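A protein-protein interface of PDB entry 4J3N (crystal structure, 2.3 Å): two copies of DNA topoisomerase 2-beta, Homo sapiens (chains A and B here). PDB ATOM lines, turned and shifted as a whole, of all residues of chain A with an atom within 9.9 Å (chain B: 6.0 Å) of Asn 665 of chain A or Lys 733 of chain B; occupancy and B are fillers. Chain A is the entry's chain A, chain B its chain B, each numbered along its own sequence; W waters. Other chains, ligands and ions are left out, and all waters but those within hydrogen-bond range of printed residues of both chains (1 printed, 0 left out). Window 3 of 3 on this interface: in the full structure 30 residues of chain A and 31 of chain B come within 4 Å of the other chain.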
ATOM      1  N   LYS A 656      35.223  -7.607  19.150  1.00  0.00           N
ATOM      2  CA  LYS A 656      34.971  -8.806  18.354  1.00  0.00           C
ATOM      3  C   LYS A 656      35.950  -8.947  17.197  1.00  0.00           C
ATOM      4  O   LYS A 656      36.518 -10.017  17.008  1.00  0.00           O
ATOM      5  CB  LYS A 656      33.543  -8.826  17.807  1.00  0.00           C
ATOM      6  CG  LYS A 656      33.170 -10.120  17.070  1.00  0.00           C
ATOM      7  CD  LYS A 656      32.723 -11.204  18.051  1.00  0.00           C
ATOM      8  CE  LYS A 656      32.470 -12.551  17.351  1.00  0.00           C
ATOM      9  NZ  LYS A 656      33.604 -12.994  16.464  1.00  0.00           N
ATOM     10  N   THR A 662      34.535 -13.514  21.871  1.00  0.00           N
ATOM     11  CA  THR A 662      33.910 -14.412  20.911  1.00  0.00           C
ATOM     12  C   THR A 662      32.539 -14.781  21.433  1.00  0.00           C
ATOM     13  O   THR A 662      32.348 -14.937  22.640  1.00  0.00           O
ATOM     14  CB  THR A 662      34.716 -15.726  20.666  1.00  0.00           C
ATOM     15  OG1 THR A 662      34.508 -16.642  21.749  1.00  0.00           O
ATOM     16  CG2 THR A 662      36.199 -15.449  20.508  1.00  0.00           C
ATOM     17  N   ILE A 663      31.584 -14.912  20.523  1.00  0.00           N
ATOM     18  CA  ILE A 663      30.250 -15.359  20.896  1.00  0.00           C
ATOM     19  C   ILE A 663      29.969 -16.720  20.262  1.00  0.00           C
ATOM     20  O   ILE A 663      29.061 -17.436  20.678  1.00  0.00           O
ATOM     21  CB  ILE A 663      29.176 -14.331  20.485  1.00  0.00           C
ATOM     22  CG1 ILE A 663      29.192 -14.099  18.976  1.00  0.00           C
ATOM     23  CG2 ILE A 663      29.418 -13.007  21.184  1.00  0.00           C
ATOM     24  CD1 ILE A 663      28.059 -13.183  18.493  1.00  0.00           C
ATOM     25  N   GLU A 664      30.776 -17.072  19.263  1.00  0.00           N
ATOM     26  CA  GLU A 664      30.572 -18.298  18.500  1.00  0.00           C
ATOM     27  C   GLU A 664      30.295 -19.499  19.386  1.00  0.00           C
ATOM     28  O   GLU A 664      31.113 -19.870  20.222  1.00  0.00           O
ATOM     29  CB  GLU A 664      31.762 -18.585  17.593  1.00  0.00           C
ATOM     30  CG  GLU A 664      31.797 -17.770  16.307  1.00  0.00           C
ATOM     31  CD  GLU A 664      32.362 -16.385  16.523  1.00  0.00           C
ATOM     32  OE1 GLU A 664      32.566 -16.032  17.700  1.00  0.00           O
ATOM     33  OE2 GLU A 664      32.605 -15.659  15.527  1.00  0.00           O
ATOM     34  N   ASN A 665      29.120 -20.085  19.189  1.00  0.00           N
ATOM     35  CA  ASN A 665      28.673 -21.286  19.892  1.00  0.00           C
ATOM     36  C   ASN A 665      28.571 -21.197  21.422  1.00  0.00           C
ATOM     37  O   ASN A 665      28.520 -22.220  22.101  1.00  0.00           O
ATOM     38  CB  ASN A 665      29.482 -22.519  19.461  1.00  0.00           C
ATOM     39  CG  ASN A 665      28.682 -23.815  19.600  1.00  0.00           C
ATOM     40  OD1 ASN A 665      29.197 -24.835  20.061  1.00  0.00           O
ATOM     41  ND2 ASN A 665      27.403 -23.764  19.222  1.00  0.00           N
ATOM     42  N   ARG A 666      28.518 -19.982  21.963  1.00  0.00           N
ATOM     43  CA  ARG A 666      28.247 -19.828  23.390  1.00  0.00           C
ATOM     44  C   ARG A 666      26.750 -19.876  23.636  1.00  0.00           C
ATOM     45  O   ARG A 666      25.970 -19.439  22.797  1.00  0.00           O
ATOM     46  CB  ARG A 666      28.799 -18.507  23.908  1.00  0.00           C
ATOM     47  CG  ARG A 666      30.238 -18.231  23.523  1.00  0.00           C
ATOM     48  CD  ARG A 666      30.716 -16.966  24.214  1.00  0.00           C
ATOM     49  NE  ARG A 666      31.291 -17.255  25.522  1.00  0.00           N
ATOM     50  CZ  ARG A 666      32.595 -17.254  25.773  1.00  0.00           C
ATOM     51  NH1 ARG A 666      33.453 -16.959  24.802  1.00  0.00           N
ATOM     52  NH2 ARG A 666      33.041 -17.534  26.990  1.00  0.00           N
ATOM     53  N   SER A 667      26.344 -20.413  24.782  1.00  0.00           N
ATOM     54  CA  SER A 667      24.935 -20.417  25.138  1.00  0.00           C
ATOM     55  C   SER A 667      24.479 -19.002  25.469  1.00  0.00           C
ATOM     56  O   SER A 667      25.298 -18.134  25.806  1.00  0.00           O
ATOM     57  CB  SER A 667      24.683 -21.319  26.343  1.00  0.00           C
ATOM     58  OG  SER A 667      25.286 -20.780  27.504  1.00  0.00           O
ATOM     59  N   LYS A 668      23.171 -18.778  25.392  1.00  0.00           N
ATOM     60  CA  LYS A 668      22.605 -17.479  25.713  1.00  0.00           C
ATOM     61  C   LYS A 668      23.022 -17.023  27.113  1.00  0.00           C
ATOM     62  O   LYS A 668      23.563 -15.928  27.270  1.00  0.00           O
ATOM     63  CB  LYS A 668      21.083 -17.498  25.571  1.00  0.00           C
ATOM     64  CG  LYS A 668      20.437 -16.119  25.663  1.00  0.00           C
ATOM     65  CD  LYS A 668      18.964 -16.198  25.320  1.00  0.00           C
ATOM     66  CE  LYS A 668      18.223 -14.908  25.635  1.00  0.00           C
ATOM     67  NZ  LYS A 668      16.764 -14.999  25.302  1.00  0.00           N
ATOM     68  N   LYS A 669      22.790 -17.863  28.121  1.00  0.00           N
ATOM     69  CA  LYS A 669      23.145 -17.511  29.500  1.00  0.00           C
ATOM     70  C   LYS A 669      24.623 -17.175  29.666  1.00  0.00           C
ATOM     71  O   LYS A 669      24.972 -16.179  30.292  1.00  0.00           O
ATOM     72  CB  LYS A 669      22.727 -18.608  30.486  1.00  0.00           C
ATOM     73  CG  LYS A 669      21.224 -18.646  30.754  1.00  0.00           C
ATOM     74  CD  LYS A 669      20.781 -19.979  31.357  1.00  0.00           C
ATOM     75  CE  LYS A 669      19.257 -20.134  31.326  1.00  0.00           C
ATOM     76  NZ  LYS A 669      18.822 -21.545  31.581  1.00  0.00           N
ATOM     77  N   ASP A 670      25.501 -17.992  29.103  1.00  0.00           N
ATOM     78  CA  ASP A 670      26.921 -17.725  29.255  1.00  0.00           C
ATOM     79  C   ASP A 670      27.310 -16.412  28.579  1.00  0.00           C
ATOM     80  O   ASP A 670      28.212 -15.710  29.036  1.00  0.00           O
ATOM     81  CB  ASP A 670      27.769 -18.893  28.731  1.00  0.00           C
ATOM     82  CG  ASP A 670      27.613 -20.158  29.579  1.00  0.00           C
ATOM     83  OD1 ASP A 670      27.434 -20.031  30.812  1.00  0.00           O
ATOM     84  OD2 ASP A 670      27.660 -21.276  29.011  1.00  0.00           O
ATOM     85  N   LEU A 671      26.621 -16.087  27.491  1.00  0.00           N
ATOM     86  CA  LEU A 671      26.931 -14.902  26.709  1.00  0.00           C
ATOM     87  C   LEU A 671      26.515 -13.628  27.448  1.00  0.00           C
ATOM     88  O   LEU A 671      27.243 -12.648  27.467  1.00  0.00           O
ATOM     89  CB  LEU A 671      26.246 -14.978  25.344  1.00  0.00           C
ATOM     90  CG  LEU A 671      26.517 -13.798  24.412  1.00  0.00           C
ATOM     91  CD1 LEU A 671      28.008 -13.589  24.276  1.00  0.00           C
ATOM     92  CD2 LEU A 671      25.875 -14.014  23.050  1.00  0.00           C
ATOM     93  N   ILE B 657      31.303 -20.647  13.269  1.00  0.00           N
ATOM     94  CA  ILE B 657      31.591 -21.097  14.624  1.00  0.00           C
ATOM     95  C   ILE B 657      32.769 -22.077  14.702  1.00  0.00           C
ATOM     96  O   ILE B 657      33.273 -22.353  15.794  1.00  0.00           O
ATOM     97  CB  ILE B 657      30.353 -21.697  15.349  1.00  0.00           C
ATOM     98  CG1 ILE B 657      29.913 -23.009  14.711  1.00  0.00           C
ATOM     99  CG2 ILE B 657      29.196 -20.706  15.388  1.00  0.00           C
ATOM    100  CD1 ILE B 657      28.757 -23.683  15.461  1.00  0.00           C
ATOM    101  N   TRP B 729      23.102 -12.986  17.070  1.00  0.00           N
ATOM    102  CA  TRP B 729      22.476 -14.033  17.873  1.00  0.00           C
ATOM    103  C   TRP B 729      22.612 -15.407  17.214  1.00  0.00           C
ATOM    104  O   TRP B 729      22.653 -16.424  17.900  1.00  0.00           O
ATOM    105  CB  TRP B 729      20.985 -13.764  18.062  1.00  0.00           C
ATOM    106  CG  TRP B 729      20.607 -12.901  19.236  1.00  0.00           C
ATOM    107  CD1 TRP B 729      19.879 -11.745  19.199  1.00  0.00           C
ATOM    108  CD2 TRP B 729      20.912 -13.138  20.616  1.00  0.00           C
ATOM    109  NE1 TRP B 729      19.717 -11.250  20.472  1.00  0.00           N
ATOM    110  CE2 TRP B 729      20.340 -12.086  21.358  1.00  0.00           C
ATOM    111  CE3 TRP B 729      21.615 -14.136  21.296  1.00  0.00           C
ATOM    112  CZ2 TRP B 729      20.456 -11.998  22.742  1.00  0.00           C
ATOM    113  CZ3 TRP B 729      21.724 -14.050  22.673  1.00  0.00           C
ATOM    114  CH2 TRP B 729      21.149 -12.986  23.380  1.00  0.00           C
ATOM    115  N   LEU B 731      24.972 -16.908  15.905  1.00  0.00           N
ATOM    116  CA  LEU B 731      26.211 -17.624  16.152  1.00  0.00           C
ATOM    117  C   LEU B 731      26.166 -18.315  17.499  1.00  0.00           C
ATOM    118  O   LEU B 731      27.102 -19.007  17.869  1.00  0.00           O
ATOM    119  CB  LEU B 731      27.409 -16.668  16.091  1.00  0.00           C
ATOM    120  CG  LEU B 731      27.611 -15.855  14.805  1.00  0.00           C
ATOM    121  CD1 LEU B 731      28.860 -14.981  14.894  1.00  0.00           C
ATOM    122  CD2 LEU B 731      27.690 -16.753  13.576  1.00  0.00           C
ATOM    123  N   THR B 732      25.075 -18.136  18.238  1.00  0.00           N
ATOM    124  CA  THR B 732      25.006 -18.692  19.591  1.00  0.00           C
ATOM    125  C   THR B 732      24.399 -20.092  19.595  1.00  0.00           C
ATOM    126  O   THR B 732      23.675 -20.469  18.676  1.00  0.00           O
ATOM    127  CB  THR B 732      24.230 -17.775  20.572  1.00  0.00           C
ATOM    128  OG1 THR B 732      22.855 -17.696  20.180  1.00  0.00           O
ATOM    129  CG2 THR B 732      24.841 -16.363  20.614  1.00  0.00           C
ATOM    130  N   LYS B 733      24.700 -20.840  20.648  1.00  0.00           N
ATOM    131  CA  LYS B 733      24.348 -22.249  20.758  1.00  0.00           C
ATOM    132  C   LYS B 733      22.905 -22.566  20.390  1.00  0.00           C
ATOM    133  O   LYS B 733      22.646 -23.332  19.461  1.00  0.00           O
ATOM    134  CB  LYS B 733      24.646 -22.758  22.176  1.00  0.00           C
ATOM    135  CG  LYS B 733      24.396 -24.251  22.362  1.00  0.00           C
ATOM    136  CD  LYS B 733      25.085 -24.783  23.608  1.00  0.00           C
ATOM    137  CE  LYS B 733      26.589 -24.500  23.573  1.00  0.00           C
ATOM    138  NZ  LYS B 733      27.283 -25.203  22.451  1.00  0.00           N
ATOM    139  N   GLU B 734      21.969 -21.996  21.139  1.00  0.00           N
ATOM    140  CA  GLU B 734      20.556 -22.251  20.909  1.00  0.00           C
ATOM    141  C   GLU B 734      20.163 -21.981  19.460  1.00  0.00           C
ATOM    142  O   GLU B 734      19.432 -22.768  18.862  1.00  0.00           O
ATOM    143  CB  GLU B 734      19.692 -21.416  21.856  1.00  0.00           C
ATOM    144  CG  GLU B 734      19.735 -21.885  23.288  1.00  0.00           C
ATOM    145  CD  GLU B 734      20.929 -21.335  24.072  1.00  0.00           C
ATOM    146  OE1 GLU B 734      21.736 -20.546  23.512  1.00  0.00           O
ATOM    147  OE2 GLU B 734      21.055 -21.704  25.262  1.00  0.00           O
ATOM    148  N   LYS B 735      20.661 -20.882  18.901  1.00  0.00           N
ATOM    149  CA  LYS B 735      20.282 -20.463  17.556  1.00  0.00           C
ATOM    150  C   LYS B 735      20.928 -21.331  16.488  1.00  0.00           C
ATOM    151  O   LYS B 735      20.352 -21.534  15.417  1.00  0.00           O
ATOM    152  CB  LYS B 735      20.649 -18.998  17.299  1.00  0.00           C
ATOM    153  CG  LYS B 735      20.136 -18.023  18.340  1.00  0.00           C
ATOM    154  CD  LYS B 735      18.629 -18.041  18.463  1.00  0.00           C
ATOM    155  CE  LYS B 735      17.959 -17.400  17.273  1.00  0.00           C
ATOM    156  NZ  LYS B 735      16.532 -17.087  17.592  1.00  0.00           N
ATOM    157  N   VAL B 736      22.134 -21.814  16.761  1.00  0.00           N
ATOM    158  CA  VAL B 736      22.776 -22.739  15.838  1.00  0.00           C
ATOM    159  C   VAL B 736      21.944 -24.009  15.724  1.00  0.00           C
ATOM    160  O   VAL B 736      21.644 -24.447  14.618  1.00  0.00           O
ATOM    161  CB  VAL B 736      24.204 -23.097  16.259  1.00  0.00           C
ATOM    162  CG1 VAL B 736      24.714 -24.273  15.437  1.00  0.00           C
ATOM    163  CG2 VAL B 736      25.108 -21.893  16.080  1.00  0.00           C
ATOM    164  N   GLU B 737      21.560 -24.573  16.871  1.00  0.00           N
ATOM    165  CA  GLU B 737      20.733 -25.767  16.910  1.00  0.00           C
ATOM    166  C   GLU B 737      19.425 -25.526  16.176  1.00  0.00           C
ATOM    167  O   GLU B 737      19.003 -26.341  15.354  1.00  0.00           O
ATOM    168  CB  GLU B 737      20.437 -26.178  18.354  1.00  0.00           C
ATOM    169  CG  GLU B 737      21.681 -26.546  19.158  1.00  0.00           C
ATOM    170  CD  GLU B 737      21.413 -26.706  20.654  1.00  0.00           C
ATOM    171  OE1 GLU B 737      20.327 -26.299  21.133  1.00  0.00           O
ATOM    172  OE2 GLU B 737      22.303 -27.239  21.357  1.00  0.00           O
ATOM    173  N   GLU B 738      18.798 -24.395  16.482  1.00  0.00           N
ATOM    174  CA  GLU B 738      17.497 -24.047  15.925  1.00  0.00           C
ATOM    175  C   GLU B 738      17.563 -23.902  14.406  1.00  0.00           C
ATOM    176  O   GLU B 738      16.677 -24.357  13.688  1.00  0.00           O
ATOM    177  CB  GLU B 738      16.969 -22.758  16.573  1.00  0.00           C
ATOM    178  CG  GLU B 738      15.622 -22.287  16.025  1.00  0.00           C
ATOM    179  CD  GLU B 738      15.225 -20.882  16.499  1.00  0.00           C
ATOM    180  OE1 GLU B 738      15.993 -20.244  17.256  1.00  0.00           O
ATOM    181  OE2 GLU B 738      14.131 -20.414  16.107  1.00  0.00           O
HETATM  182  O   HOH W   1      21.088 -20.266  27.830  1.00  0.00           O
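No position is printed for both chains.
Printed residues of chain B that touch a printed residue of chain A: Ile 657, Trp 729, Leu 731, Thr 732, Lys 733 and Glu 734. Hydrophobic or aromatic side chains of chain B within 4 Å of the printed part of chain A: Ile 657, Trp 729 and Leu 731. Along chain B the printed residues that touch a printed residue of chain A span positions 657 to 734. Printed residues of chain A that touch a printed residue of chain B: Ile 663, Glu 664, Asn 665, Arg 666, Ser 667, Lys 668 and Leu 671. Among the printed residues, no Asp or Glu carboxylate lies within 4 Å of a Lys or Arg side-chain nitrogen of the other chain.
Among the printed residues, merely in contact across the chains: Ile 663 of chain A with Leu 731 of chain B, Glu 664 of chain A with Ile 657 of chain B, Glu 664 of chain A with Leu 731 of chain B, Asn 665 of chain A with Ile 657 of chain B, Arg 666 of chain A with Thr 732 of chain B, Ser 667 of chain A with Lys 733 of chain B, Ser 667 of chain A with Glu 734 of chain B, Lys 668 of chain A with Trp 729 of chain B and Leu 671 of chain A with Thr 732 of chain B.
The side-chain hydroxyl (OG1) of Thr 732 of chain B is in hydrogen-bond range of the backbone carbonyl oxygen (O) of Trp 729 of chain B. The backbone carbonyl oxygen (O) of Thr 662 of chain A lies close to the guanidinium group (NH1) of Arg 666 of chain A, 3.2 Å away. The side-chain amino group (NZ) of Lys 656 of chain A lies within salt-bridge range of the side-chain carboxylate (OE2) of Glu 664 of chain A, 3.0 Å away. The side-chain carboxylate (OD2) of Asp 670 of chain A is in hydrogen-bond range of the side-chain hydroxyl (OG) of Ser 667 of chain A, at 2.9 Å.
N of Lys 733 of chain B is in hydrogen-bond range of O of Arg 666 of chain A (2.9 Å). The backbone NH of Asn 665 of chain A sits at hydrogen-bond distance from the backbone carbonyl oxygen of Leu 731 of chain B. The side-chain amide oxygen of Asn 665 of chain A lies within hydrogen-bond range of the side-chain amino group of Lys 733 of chain B (3.1 Å). N of Lys 668 of chain A is in hydrogen-bond range of OE1 of Glu 734 of chain B, at 3.0 Å.
Water W1 lies within hydrogen-bond range of OE2 of Glu 734 of chain B (2.9 Å) and N of Lys 669 of chain A (3.0 Å).
Printed residues of chain B within 4 Å of Glu 664 of chain A: Ile 657 and Leu 731. Of chain B, only Ile 657, Leu 731 and Lys 733 come within 4 Å of Asn 665 of chain A. Of the printed residues of chain B, Ser 667 of chain A touches Lys 733 (3.8 Å) and Glu 734 (3.6 Å). Of the printed residues of chain B, Lys 668 of chain A touches Trp 729 and Glu 734. Of the printed residues of chain A, Trp 729 of chain B touches Lys 668. Of chain A, only Arg 666 (3.3 Å) and Leu 671 (3.5 Å) come within 4 Å of Thr 732 of chain B. Lys 733 of chain B touches just these residues of chain A: Asn 665 (3.1 Å), Arg 666 (2.9 Å) and Ser 667 (3.8 Å). No residue of chain A comes within 4 Å of Val 736 of chain B. Glu 737 of chain B touches none of the printed residues of chain A. Glu 738 of chain B touches none of the printed residues of chain A. The nearest residue of chain A that does not touch Lys 733 of chain B is Lys 668 of chain A (5.3 Å).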
